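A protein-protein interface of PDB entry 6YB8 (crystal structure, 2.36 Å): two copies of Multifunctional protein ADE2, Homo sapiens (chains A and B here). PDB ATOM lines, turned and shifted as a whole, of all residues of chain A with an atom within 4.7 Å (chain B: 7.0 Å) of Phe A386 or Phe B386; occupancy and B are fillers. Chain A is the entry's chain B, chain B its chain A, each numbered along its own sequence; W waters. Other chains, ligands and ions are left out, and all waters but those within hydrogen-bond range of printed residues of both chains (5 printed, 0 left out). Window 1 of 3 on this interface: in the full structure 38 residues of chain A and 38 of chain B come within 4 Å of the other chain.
Pro A346 touches Ile B390, and with the chains exchanged Ile A390 touches Pro B346. Gly A373 touches Phe B386, and with the chains exchanged Phe A386 touches Gly B373. Ser A375 touches Val B377, and with the chains exchanged Val A377 touches Ser B375. Gln A389 touches Gly B373, but with the chains exchanged Gly A373 does not touch Gln B389 (4.01 Å). Of the 25 pairs that touch across the chains among the printed residues, 21 have their exchanged pair printed and touching as well.
The side-chain amide oxygen (OE1) of Gln A385 sits at hydrogen-bond distance from the backbone NH (N) of Leu B372. OE1 of Gln A385 sits at hydrogen-bond distance from N of Gly B373 (3.4 Å). The side-chain amide oxygen (OE1) of Gln B385 is in hydrogen-bond range of the backbone NH (N) of Gly A373 (3.4 Å).
Water W4 bridges the side-chain amide oxygen (OE1) of Gln B389 and the backbone NH (N) of Val A347. Water W2 lies within hydrogen-bond range of NE2 of Gln B389 (2.6 Å) and N of Gly A373 (2.9 Å). Water W3 lies within hydrogen-bond range of OE1 of Gln A389 (2.6 Å), OG of Ser B340 (2.9 Å), N of Cys B374 (3.3 Å) and N of Val B347 (3.3 Å). Water W1 lies within hydrogen-bond range of O of Gln A389 (2.7 Å) and O of Ala B344 (2.8 Å). Water W5 lies within hydrogen-bond range of the backbone carbonyl oxygen of Ser B340 (2.9 Å), the backbone carbonyl oxygen of Tyr B345 (2.9 Å) and the side-chain amide nitrogen of Gln A389 (3.1 Å).
Of the 15 printed residues of chain A, 10 touch a printed residue of chain B. Hydrophobic or aromatic side chains of chain A that line the printed part of chain B: Pro A346, Val A377, Phe A386 and Ile A390. Among the printed residues, no Asp or Glu carboxylate lies within 4 Å of a Lys or Arg side-chain nitrogen of the other chain.
Phe A386 touches just these residues of chain B: Pro B346 (3.9 Å), Val B347 (3.5 Å), Gly B373 (3.2 Å), Ser B375 (3.2 Å) and Phe B386 (3.2 Å). Phe B386 touches just these residues of chain A: Pro A346 (3.8 Å), Val A347 (3.6 Å), Gly A373 (3.0 Å), Ser A375 (3.2 Å) and Phe A386 (3.2 Å). Printed residues of chain A within 4 Å of Val B377: Ser A375. Of the printed residues of chain A, Ser B375 touches Ser A375 (3.9 Å), Val A377 (3.8 Å) and Phe A386 (3.2 Å). Ala B388 touches none of the printed residues of chain A. The nearest residue of chain B that does not touch Phe A386 is Ile B348 (4.3 Å).
N of Ser B375 lies within hydrogen-bond range of O of Val B347, at 3.3 Å. The backbone carbonyl oxygen (O) of Val A347 lies within hydrogen-bond range of the backbone NH (N) of Ser A375, 3.3 Å away.
Pro A346 touches Phe B386. Gln B389 touches Pro A346. O of Val A347 touches CE1 of Phe B386, at 3.6 Å. Gly B382 touches Gly A373. Ser A375 touches Ser B375. Ser A375 touches Phe B386. Phe A386 touches Val B347 (CE1 to O, 3.5 Å). Phe A386 touches Phe B386 (CE2 to CE2, 3.2 Å). N of Ile A390 touches CG of Pro B346, 3.95 Å away. CG2 of Ile A390 touches CG2 of Ile B390 (3.7 Å).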
ATOM      1  N   PRO A 346       5.396  -0.089  25.626  1.00  0.00           N
ATOM      2  CA  PRO A 346       6.257  -1.236  25.832  1.00  0.00           C
ATOM      3  C   PRO A 346       6.742  -1.376  27.282  1.00  0.00           C
ATOM      4  O   PRO A 346       7.072  -0.397  27.925  1.00  0.00           O
ATOM      5  CB  PRO A 346       7.459  -0.981  24.904  1.00  0.00           C
ATOM      6  CG  PRO A 346       7.062   0.176  24.025  1.00  0.00           C
ATOM      7  CD  PRO A 346       6.017   0.953  24.801  1.00  0.00           C
ATOM      8  N   VAL A 347       6.813  -2.614  27.741  1.00  0.00           N
ATOM      9  CA  VAL A 347       7.409  -2.995  29.048  1.00  0.00           C
ATOM     10  C   VAL A 347       8.512  -4.024  28.817  1.00  0.00           C
ATOM     11  O   VAL A 347       8.282  -5.018  28.126  1.00  0.00           O
ATOM     12  CB  VAL A 347       6.346  -3.527  30.006  1.00  0.00           C
ATOM     13  CG1 VAL A 347       6.962  -3.916  31.323  1.00  0.00           C
ATOM     14  CG2 VAL A 347       5.297  -2.470  30.233  1.00  0.00           C
ATOM     15  N   ILE A 348       9.671  -3.749  29.383  1.00  0.00           N
ATOM     16  CA  ILE A 348      10.869  -4.620  29.359  1.00  0.00           C
ATOM     17  C   ILE A 348      11.109  -5.079  30.787  1.00  0.00           C
ATOM     18  O   ILE A 348      11.304  -4.204  31.675  1.00  0.00           O
ATOM     19  CB  ILE A 348      12.100  -3.852  28.844  1.00  0.00           C
ATOM     20  CG1 ILE A 348      11.888  -3.259  27.449  1.00  0.00           C
ATOM     21  CG2 ILE A 348      13.330  -4.744  28.867  1.00  0.00           C
ATOM     22  CD1 ILE A 348      12.988  -2.282  27.034  1.00  0.00           C
ATOM     23  N   GLY A 373       2.620  -8.647  25.876  1.00  0.00           N
ATOM     24  CA  GLY A 373       3.777  -8.410  24.991  1.00  0.00           C
ATOM     25  C   GLY A 373       5.088  -8.218  25.738  1.00  0.00           C
ATOM     26  O   GLY A 373       6.092  -7.968  25.024  1.00  0.00           O
ATOM     27  N   SER A 375       8.631  -8.087  27.052  1.00  0.00           N
ATOM     28  CA  SER A 375       9.950  -8.604  26.629  1.00  0.00           C
ATOM     29  C   SER A 375      10.879  -8.786  27.840  1.00  0.00           C
ATOM     30  O   SER A 375      10.591  -8.295  28.949  1.00  0.00           O
ATOM     31  CB  SER A 375      10.568  -7.706  25.583  1.00  0.00           C
ATOM     32  OG  SER A 375      10.947  -6.451  26.130  1.00  0.00           O
ATOM     33  N   VAL A 377      15.112  -8.469  28.618  1.00  0.00           N
ATOM     34  CA  VAL A 377      16.540  -8.153  28.362  1.00  0.00           C
ATOM     35  C   VAL A 377      17.287  -8.302  29.688  1.00  0.00           C
ATOM     36  O   VAL A 377      17.002  -7.503  30.591  1.00  0.00           O
ATOM     37  CB  VAL A 377      16.745  -6.746  27.786  1.00  0.00           C
ATOM     38  CG1 VAL A 377      18.201  -6.555  27.397  1.00  0.00           C
ATOM     39  CG2 VAL A 377      15.828  -6.469  26.609  1.00  0.00           C
ATOM     40  N   GLY A 382      22.048  -3.286  28.170  1.00  0.00           N
ATOM     41  CA  GLY A 382      21.176  -3.788  27.099  1.00  0.00           C
ATOM     42  C   GLY A 382      19.742  -3.276  27.180  1.00  0.00           C
ATOM     43  O   GLY A 382      19.155  -3.001  26.114  1.00  0.00           O
ATOM     44  N   SER A 383      19.151  -3.209  28.362  1.00  0.00           N
ATOM     45  CA  SER A 383      17.783  -2.684  28.588  1.00  0.00           C
ATOM     46  C   SER A 383      17.673  -1.324  27.908  1.00  0.00           C
ATOM     47  O   SER A 383      16.769  -1.067  27.124  1.00  0.00           O
ATOM     48  CB  SER A 383      17.539  -2.446  30.057  1.00  0.00           C
ATOM     49  OG  SER A 383      17.463  -3.646  30.733  1.00  0.00           O
ATOM     50  N   ALA A 384      18.614  -0.472  28.261  1.00  0.00           N
ATOM     51  CA  ALA A 384      18.670   0.938  27.835  1.00  0.00           C
ATOM     52  C   ALA A 384      18.869   0.962  26.323  1.00  0.00           C
ATOM     53  O   ALA A 384      18.133   1.639  25.635  1.00  0.00           O
ATOM     54  CB  ALA A 384      19.777   1.655  28.587  1.00  0.00           C
ATOM     55  N   GLN A 385      19.774   0.138  25.834  1.00  0.00           N
ATOM     56  CA  GLN A 385      20.046   0.016  24.389  1.00  0.00           C
ATOM     57  C   GLN A 385      18.761  -0.407  23.682  1.00  0.00           C
ATOM     58  O   GLN A 385      18.412   0.185  22.638  1.00  0.00           O
ATOM     59  CB  GLN A 385      21.196  -0.954  24.155  1.00  0.00           C
ATOM     60  CG  GLN A 385      21.699  -0.882  22.726  1.00  0.00           C
ATOM     61  CD  GLN A 385      22.849  -1.800  22.437  1.00  0.00           C
ATOM     62  OE1 GLN A 385      23.291  -2.537  23.312  1.00  0.00           O
ATOM     63  NE2 GLN A 385      23.307  -1.758  21.194  1.00  0.00           N
ATOM     64  N   PHE A 386      18.052  -1.392  24.222  1.00  0.00           N
ATOM     65  CA  PHE A 386      16.811  -1.841  23.578  1.00  0.00           C
ATOM     66  C   PHE A 386      15.848  -0.662  23.593  1.00  0.00           C
ATOM     67  O   PHE A 386      15.197  -0.393  22.561  1.00  0.00           O
ATOM     68  CB  PHE A 386      16.224  -3.080  24.236  1.00  0.00           C
ATOM     69  CG  PHE A 386      15.149  -3.680  23.381  1.00  0.00           C
ATOM     70  CD1 PHE A 386      15.438  -4.145  22.116  1.00  0.00           C
ATOM     71  CD2 PHE A 386      13.838  -3.703  23.801  1.00  0.00           C
ATOM     72  CE1 PHE A 386      14.454  -4.702  21.321  1.00  0.00           C
ATOM     73  CE2 PHE A 386      12.845  -4.189  22.975  1.00  0.00           C
ATOM     74  CZ  PHE A 386      13.159  -4.699  21.738  1.00  0.00           C
ATOM     75  N   ALA A 387      15.774   0.052  24.703  1.00  0.00           N
ATOM     76  CA  ALA A 387      14.829   1.191  24.820  1.00  0.00           C
ATOM     77  C   ALA A 387      15.244   2.259  23.806  1.00  0.00           C
ATOM     78  O   ALA A 387      14.383   2.755  23.109  1.00  0.00           O
ATOM     79  CB  ALA A 387      14.786   1.711  26.227  1.00  0.00           C
ATOM     80  N   ALA A 388      16.538   2.492  23.633  1.00  0.00           N
ATOM     81  CA  ALA A 388      17.041   3.444  22.619  1.00  0.00           C
ATOM     82  C   ALA A 388      16.609   2.990  21.233  1.00  0.00           C
ATOM     83  O   ALA A 388      16.137   3.831  20.452  1.00  0.00           O
ATOM     84  CB  ALA A 388      18.529   3.610  22.701  1.00  0.00           C
ATOM     85  N   GLN A 389      16.722   1.697  20.953  1.00  0.00           N
ATOM     86  CA  GLN A 389      16.384   1.150  19.618  1.00  0.00           C
ATOM     87  C   GLN A 389      14.905   1.440  19.333  1.00  0.00           C
ATOM     88  O   GLN A 389      14.577   1.842  18.176  1.00  0.00           O
ATOM     89  CB  GLN A 389      16.758  -0.332  19.545  1.00  0.00           C
ATOM     90  CG  GLN A 389      18.257  -0.572  19.369  1.00  0.00           C
ATOM     91  CD  GLN A 389      18.687  -1.982  19.711  1.00  0.00           C
ATOM     92  OE1 GLN A 389      17.922  -2.798  20.221  1.00  0.00           O
ATOM     93  NE2 GLN A 389      19.952  -2.274  19.477  1.00  0.00           N
ATOM     94  N   ILE A 390      14.033   1.245  20.320  1.00  0.00           N
ATOM     95  CA  ILE A 390      12.584   1.538  20.131  1.00  0.00           C
ATOM     96  C   ILE A 390      12.421   3.038  19.819  1.00  0.00           C
ATOM     97  O   ILE A 390      11.718   3.409  18.890  1.00  0.00           O
ATOM     98  CB  ILE A 390      11.846   1.135  21.412  1.00  0.00           C
ATOM     99  CG1 ILE A 390      11.904  -0.364  21.644  1.00  0.00           C
ATOM    100  CG2 ILE A 390      10.429   1.673  21.441  1.00  0.00           C
ATOM    101  CD1 ILE A 390      11.486  -0.763  23.046  1.00  0.00           C
ATOM    102  N   PHE B 291      -3.090  -5.743  14.415  1.00  0.00           N
ATOM    103  CA  PHE B 291      -2.672  -4.379  14.856  1.00  0.00           C
ATOM    104  C   PHE B 291      -2.534  -3.419  13.662  1.00  0.00           C
ATOM    105  O   PHE B 291      -2.189  -2.278  13.897  1.00  0.00           O
ATOM    106  CB  PHE B 291      -1.390  -4.440  15.683  1.00  0.00           C
ATOM    107  CG  PHE B 291      -1.585  -5.126  17.004  1.00  0.00           C
ATOM    108  CD1 PHE B 291      -2.296  -4.516  18.006  1.00  0.00           C
ATOM    109  CD2 PHE B 291      -1.111  -6.402  17.218  1.00  0.00           C
ATOM    110  CE1 PHE B 291      -2.513  -5.169  19.201  1.00  0.00           C
ATOM    111  CE2 PHE B 291      -1.329  -7.055  18.413  1.00  0.00           C
ATOM    112  CZ  PHE B 291      -2.025  -6.433  19.397  1.00  0.00           C
ATOM    113  N   VAL B 324      10.722  -3.185  12.780  1.00  0.00           N
ATOM    114  CA  VAL B 324      11.083  -4.114  13.876  1.00  0.00           C
ATOM    115  C   VAL B 324      11.413  -5.471  13.252  1.00  0.00           C
ATOM    116  O   VAL B 324      10.616  -5.954  12.502  1.00  0.00           O
ATOM    117  CB  VAL B 324       9.938  -4.203  14.896  1.00  0.00           C
ATOM    118  CG1 VAL B 324      10.221  -5.299  15.903  1.00  0.00           C
ATOM    119  CG2 VAL B 324       9.761  -2.880  15.626  1.00  0.00           C
ATOM    120  N   SER B 340      20.928  -8.241  15.781  1.00  0.00           N
ATOM    121  CA  SER B 340      20.925  -7.239  16.864  1.00  0.00           C
ATOM    122  C   SER B 340      22.211  -6.402  16.823  1.00  0.00           C
ATOM    123  O   SER B 340      22.180  -5.191  17.117  1.00  0.00           O
ATOM    124  CB  SER B 340      20.760  -7.909  18.182  1.00  0.00           C
ATOM    125  OG  SER B 340      20.608  -6.909  19.163  1.00  0.00           O
ATOM    126  N   ALA B 344      20.590  -0.678  14.057  1.00  0.00           N
ATOM    127  CA  ALA B 344      20.114   0.280  15.069  1.00  0.00           C
ATOM    128  C   ALA B 344      18.624   0.084  15.345  1.00  0.00           C
ATOM    129  O   ALA B 344      18.139   0.606  16.390  1.00  0.00           O
ATOM    130  CB  ALA B 344      20.360   1.671  14.579  1.00  0.00           C
ATOM    131  N   TYR B 345      17.912  -0.635  14.475  1.00  0.00           N
ATOM    132  CA  TYR B 345      16.465  -0.932  14.672  1.00  0.00           C
ATOM    133  C   TYR B 345      16.322  -2.009  15.763  1.00  0.00           C
ATOM    134  O   TYR B 345      17.197  -2.858  16.009  1.00  0.00           O
ATOM    135  CB  TYR B 345      15.801  -1.375  13.356  1.00  0.00           C
ATOM    136  CG  TYR B 345      15.561  -0.317  12.298  1.00  0.00           C
ATOM    137  CD1 TYR B 345      15.411   1.027  12.599  1.00  0.00           C
ATOM    138  CD2 TYR B 345      15.424  -0.669  10.973  1.00  0.00           C
ATOM    139  CE1 TYR B 345      15.133   1.979  11.627  1.00  0.00           C
ATOM    140  CE2 TYR B 345      15.086   0.259   9.992  1.00  0.00           C
ATOM    141  CZ  TYR B 345      14.955   1.599  10.317  1.00  0.00           C
ATOM    142  OH  TYR B 345      14.710   2.526   9.338  1.00  0.00           O
ATOM    143  N   PRO B 346      15.172  -2.070  16.443  1.00  0.00           N
ATOM    144  CA  PRO B 346      14.981  -3.134  17.425  1.00  0.00           C
ATOM    145  C   PRO B 346      14.963  -4.530  16.775  1.00  0.00           C
ATOM    146  O   PRO B 346      14.386  -4.696  15.669  1.00  0.00           O
ATOM    147  CB  PRO B 346      13.600  -2.834  18.034  1.00  0.00           C
ATOM    148  CG  PRO B 346      13.231  -1.429  17.519  1.00  0.00           C
ATOM    149  CD  PRO B 346      13.994  -1.224  16.236  1.00  0.00           C
ATOM    150  N   VAL B 347      15.489  -5.514  17.513  1.00  0.00           N
ATOM    151  CA  VAL B 347      15.382  -6.952  17.163  1.00  0.00           C
ATOM    152  C   VAL B 347      14.795  -7.711  18.343  1.00  0.00           C
ATOM    153  O   VAL B 347      15.284  -7.557  19.467  1.00  0.00           O
ATOM    154  CB  VAL B 347      16.757  -7.536  16.808  1.00  0.00           C
ATOM    155  CG1 VAL B 347      16.625  -9.004  16.458  1.00  0.00           C
ATOM    156  CG2 VAL B 347      17.398  -6.768  15.676  1.00  0.00           C
ATOM    157  N   ILE B 348      13.825  -8.555  18.057  1.00  0.00           N
ATOM    158  CA  ILE B 348      13.145  -9.441  19.028  1.00  0.00           C
ATOM    159  C   ILE B 348      13.437 -10.864  18.577  1.00  0.00           C
ATOM    160  O   ILE B 348      13.069 -11.221  17.428  1.00  0.00           O
ATOM    161  CB  ILE B 348      11.626  -9.207  19.023  1.00  0.00           C
ATOM    162  CG1 ILE B 348      11.237  -7.763  19.347  1.00  0.00           C
ATOM    163  CG2 ILE B 348      10.955 -10.180  19.968  1.00  0.00           C
ATOM    164  CD1 ILE B 348       9.777  -7.447  19.032  1.00  0.00           C
ATOM    165  N   LEU B 372      24.749  -5.589  22.707  1.00  0.00           N
ATOM    166  CA  LEU B 372      23.562  -6.215  22.053  1.00  0.00           C
ATOM    167  C   LEU B 372      22.306  -5.890  22.874  1.00  0.00           C
ATOM    168  O   LEU B 372      22.215  -6.312  24.054  1.00  0.00           O
ATOM    169  CB  LEU B 372      23.774  -7.720  21.869  1.00  0.00           C
ATOM    170  CG  LEU B 372      24.376  -8.155  20.521  1.00  0.00           C
ATOM    171  CD1 LEU B 372      25.544  -7.309  20.065  1.00  0.00           C
ATOM    172  CD2 LEU B 372      24.827  -9.605  20.562  1.00  0.00           C
ATOM    173  N   GLY B 373      21.393  -5.137  22.252  1.00  0.00           N
ATOM    174  CA  GLY B 373      20.067  -4.768  22.780  1.00  0.00           C
ATOM    175  C   GLY B 373      19.026  -5.862  22.634  1.00  0.00           C
ATOM    176  O   GLY B 373      17.985  -5.711  23.297  1.00  0.00           O
ATOM    177  N   CYS B 374      19.286  -6.925  21.846  1.00  0.00           N
ATOM    178  CA  CYS B 374      18.326  -8.020  21.486  1.00  0.00           C
ATOM    179  C   CYS B 374      17.457  -8.464  22.689  1.00  0.00           C
ATOM    180  O   CYS B 374      18.020  -8.936  23.711  1.00  0.00           O
ATOM    181  CB  CYS B 374      19.070  -9.243  20.947  1.00  0.00           C
ATOM    182  SG  CYS B 374      18.031 -10.317  19.917  1.00  0.00           S
ATOM    183  N   SER B 375      16.128  -8.343  22.558  1.00  0.00           N
ATOM    184  CA  SER B 375      15.099  -8.816  23.528  1.00  0.00           C
ATOM    185  C   SER B 375      14.618 -10.220  23.173  1.00  0.00           C
ATOM    186  O   SER B 375      14.852 -10.716  22.038  1.00  0.00           O
ATOM    187  CB  SER B 375      13.907  -7.860  23.613  1.00  0.00           C
ATOM    188  OG  SER B 375      13.171  -7.809  22.385  1.00  0.00           O
ATOM    189  N   THR B 376      13.946 -10.843  24.124  1.00  0.00           N
ATOM    190  CA  THR B 376      13.314 -12.160  23.909  1.00  0.00           C
ATOM    191  C   THR B 376      11.854 -12.099  24.338  1.00  0.00           C
ATOM    192  O   THR B 376      11.564 -11.537  25.409  1.00  0.00           O
ATOM    193  CB  THR B 376      14.106 -13.288  24.569  1.00  0.00           C
ATOM    194  OG1 THR B 376      15.473 -13.044  24.239  1.00  0.00           O
ATOM    195  CG2 THR B 376      13.662 -14.649  24.073  1.00  0.00           C
ATOM    196  N   VAL B 377      10.982 -12.529  23.426  1.00  0.00           N
ATOM    197  CA  VAL B 377       9.531 -12.762  23.645  1.00  0.00           C
ATOM    198  C   VAL B 377       9.213 -14.160  23.117  1.00  0.00           C
ATOM    199  O   VAL B 377       9.342 -14.379  21.893  1.00  0.00           O
ATOM    200  CB  VAL B 377       8.690 -11.707  22.923  1.00  0.00           C
ATOM    201  CG1 VAL B 377       7.212 -11.943  23.140  1.00  0.00           C
ATOM    202  CG2 VAL B 377       9.074 -10.287  23.317  1.00  0.00           C
ATOM    203  N   GLU B 381       2.346 -14.609  19.114  1.00  0.00           N
ATOM    204  CA  GLU B 381       1.344 -13.511  19.214  1.00  0.00           C
ATOM    205  C   GLU B 381       1.915 -12.387  20.103  1.00  0.00           C
ATOM    206  O   GLU B 381       1.805 -11.201  19.764  1.00  0.00           O
ATOM    207  CB  GLU B 381       0.038 -14.016  19.828  1.00  0.00           C
ATOM    208  CG  GLU B 381      -0.742 -15.003  18.970  1.00  0.00           C
ATOM    209  CD  GLU B 381      -0.259 -16.454  18.979  1.00  0.00           C
ATOM    210  OE1 GLU B 381       0.477 -16.844  19.926  1.00  0.00           O
ATOM    211  OE2 GLU B 381      -0.611 -17.196  18.016  1.00  0.00           O
ATOM    212  N   GLY B 382       2.549 -12.745  21.208  1.00  0.00           N
ATOM    213  CA  GLY B 382       3.284 -11.783  22.048  1.00  0.00           C
ATOM    214  C   GLY B 382       4.340 -10.973  21.282  1.00  0.00           C
ATOM    215  O   GLY B 382       4.542  -9.773  21.600  1.00  0.00           O
ATOM    216  N   SER B 383       5.043 -11.569  20.336  1.00  0.00           N
ATOM    217  CA  SER B 383       6.161 -10.863  19.681  1.00  0.00           C
ATOM    218  C   SER B 383       5.553  -9.775  18.797  1.00  0.00           C
ATOM    219  O   SER B 383       6.006  -8.614  18.870  1.00  0.00           O
ATOM    220  CB  SER B 383       7.132 -11.812  19.018  1.00  0.00           C
ATOM    221  OG  SER B 383       6.575 -12.433  17.871  1.00  0.00           O
ATOM    222  N   ALA B 384       4.433 -10.079  18.156  1.00  0.00           N
ATOM    223  CA  ALA B 384       3.671  -9.096  17.354  1.00  0.00           C
ATOM    224  C   ALA B 384       3.142  -8.000  18.280  1.00  0.00           C
ATOM    225  O   ALA B 384       3.318  -6.801  17.979  1.00  0.00           O
ATOM    226  CB  ALA B 384       2.575  -9.770  16.580  1.00  0.00           C
ATOM    227  N   GLN B 385       2.568  -8.391  19.405  1.00  0.00           N
ATOM    228  CA  GLN B 385       2.055  -7.398  20.385  1.00  0.00           C
ATOM    229  C   GLN B 385       3.216  -6.505  20.871  1.00  0.00           C
ATOM    230  O   GLN B 385       3.045  -5.242  20.970  1.00  0.00           O
ATOM    231  CB  GLN B 385       1.393  -8.128  21.550  1.00  0.00           C
ATOM    232  CG  GLN B 385       0.628  -7.197  22.461  1.00  0.00           C
ATOM    233  CD  GLN B 385      -0.100  -7.931  23.544  1.00  0.00           C
ATOM    234  OE1 GLN B 385       0.076  -9.122  23.692  1.00  0.00           O
ATOM    235  NE2 GLN B 385      -0.873  -7.199  24.329  1.00  0.00           N
ATOM    236  N   PHE B 386       4.379  -7.091  21.158  1.00  0.00           N
ATOM    237  CA  PHE B 386       5.497  -6.256  21.594  1.00  0.00           C
ATOM    238  C   PHE B 386       5.833  -5.298  20.441  1.00  0.00           C
ATOM    239  O   PHE B 386       6.090  -4.088  20.677  1.00  0.00           O
ATOM    240  CB  PHE B 386       6.695  -7.069  22.049  1.00  0.00           C
ATOM    241  CG  PHE B 386       7.685  -6.206  22.770  1.00  0.00           C
ATOM    242  CD1 PHE B 386       7.341  -5.516  23.917  1.00  0.00           C
ATOM    243  CD2 PHE B 386       8.944  -6.018  22.256  1.00  0.00           C
ATOM    244  CE1 PHE B 386       8.250  -4.683  24.553  1.00  0.00           C
ATOM    245  CE2 PHE B 386       9.854  -5.201  22.887  1.00  0.00           C
ATOM    246  CZ  PHE B 386       9.497  -4.517  24.024  1.00  0.00           C
ATOM    247  N   ALA B 387       5.822  -5.798  19.216  1.00  0.00           N
ATOM    248  CA  ALA B 387       6.226  -4.958  18.066  1.00  0.00           C
ATOM    249  C   ALA B 387       5.176  -3.851  17.930  1.00  0.00           C
ATOM    250  O   ALA B 387       5.543  -2.730  17.721  1.00  0.00           O
ATOM    251  CB  ALA B 387       6.392  -5.798  16.819  1.00  0.00           C
ATOM    252  N   ALA B 388       3.908  -4.157  18.152  1.00  0.00           N
ATOM    253  CA  ALA B 388       2.835  -3.145  18.125  1.00  0.00           C
ATOM    254  C   ALA B 388       3.095  -2.095  19.202  1.00  0.00           C
ATOM    255  O   ALA B 388       2.944  -0.911  18.910  1.00  0.00           O
ATOM    256  CB  ALA B 388       1.484  -3.783  18.296  1.00  0.00           C
ATOM    257  N   GLN B 389       3.490  -2.510  20.400  1.00  0.00           N
ATOM    258  CA  GLN B 389       3.700  -1.555  21.514  1.00  0.00           C
ATOM    259  C   GLN B 389       4.812  -0.581  21.101  1.00  0.00           C
ATOM    260  O   GLN B 389       4.701   0.638  21.384  1.00  0.00           O
ATOM    261  CB  GLN B 389       3.986  -2.297  22.815  1.00  0.00           C
ATOM    262  CG  GLN B 389       2.754  -2.932  23.429  1.00  0.00           C
ATOM    263  CD  GLN B 389       3.032  -4.053  24.402  1.00  0.00           C
ATOM    264  OE1 GLN B 389       4.176  -4.427  24.688  1.00  0.00           O
ATOM    265  NE2 GLN B 389       1.953  -4.669  24.853  1.00  0.00           N
ATOM    266  N   ILE B 390       5.852  -1.071  20.435  1.00  0.00           N
ATOM    267  CA  ILE B 390       6.950  -0.189  19.952  1.00  0.00           C
ATOM    268  C   ILE B 390       6.368   0.821  18.943  1.00  0.00           C
ATOM    269  O   ILE B 390       6.621   2.047  19.060  1.00  0.00           O
ATOM    270  CB  ILE B 390       8.057  -1.059  19.343  1.00  0.00           C
ATOM    271  CG1 ILE B 390       8.685  -1.928  20.422  1.00  0.00           C
ATOM    272  CG2 ILE B 390       9.062  -0.222  18.588  1.00  0.00           C
ATOM    273  CD1 ILE B 390       9.570  -3.020  19.887  1.00  0.00           C
ATOM    274  N   PHE B 391       5.596   0.356  17.962  1.00  0.00           N
ATOM    275  CA  PHE B 391       5.038   1.257  16.931  1.00  0.00           C
ATOM    276  C   PHE B 391       3.993   2.198  17.535  1.00  0.00           C
ATOM    277  O   PHE B 391       3.810   3.330  17.026  1.00  0.00           O
ATOM    278  CB  PHE B 391       4.512   0.423  15.780  1.00  0.00           C
ATOM    279  CG  PHE B 391       5.623  -0.087  14.917  1.00  0.00           C
ATOM    280  CD1 PHE B 391       6.529   0.793  14.338  1.00  0.00           C
ATOM    281  CD2 PHE B 391       5.801  -1.443  14.705  1.00  0.00           C
ATOM    282  CE1 PHE B 391       7.557   0.321  13.524  1.00  0.00           C
ATOM    283  CE2 PHE B 391       6.832  -1.913  13.909  1.00  0.00           C
ATOM    284  CZ  PHE B 391       7.689  -1.030  13.307  1.00  0.00           C
ATOM    285  N   GLY B 392       3.341   1.771  18.612  1.00  0.00           N
ATOM    286  CA  GLY B 392       2.289   2.577  19.274  1.00  0.00           C
ATOM    287  C   GLY B 392       2.857   3.843  19.900  1.00  0.00           C
ATOM    288  O   GLY B 392       2.094   4.785  20.155  1.00  0.00           O
ATOM    289  N   LEU B 402      -4.139  -1.341  20.770  1.00  0.00           N
ATOM    290  CA  LEU B 402      -3.558  -1.958  22.003  1.00  0.00           C
ATOM    291  C   LEU B 402      -4.432  -1.552  23.208  1.00  0.00           C
ATOM    292  O   LEU B 402      -4.745  -2.395  24.068  1.00  0.00           O
ATOM    293  CB  LEU B 402      -2.107  -1.501  22.178  1.00  0.00           C
ATOM    294  CG  LEU B 402      -1.102  -2.114  21.206  1.00  0.00           C
ATOM    295  CD1 LEU B 402       0.121  -1.247  21.076  1.00  0.00           C
ATOM    296  CD2 LEU B 402      -0.698  -3.520  21.622  1.00  0.00           C
HETATM  297  O   HOH W   1      16.051   2.442  15.972  1.00  0.00           O
HETATM  298  O   HOH W   2       1.454  -6.219  26.844  1.00  0.00           O
HETATM  299  O   HOH W   3      18.255  -5.180  19.267  1.00  0.00           O
HETATM  300  O   HOH W   4       4.772  -5.027  27.033  1.00  0.00           O
HETATM  301  O   HOH W   5      19.417  -4.385  17.204  1.00  0.00           O
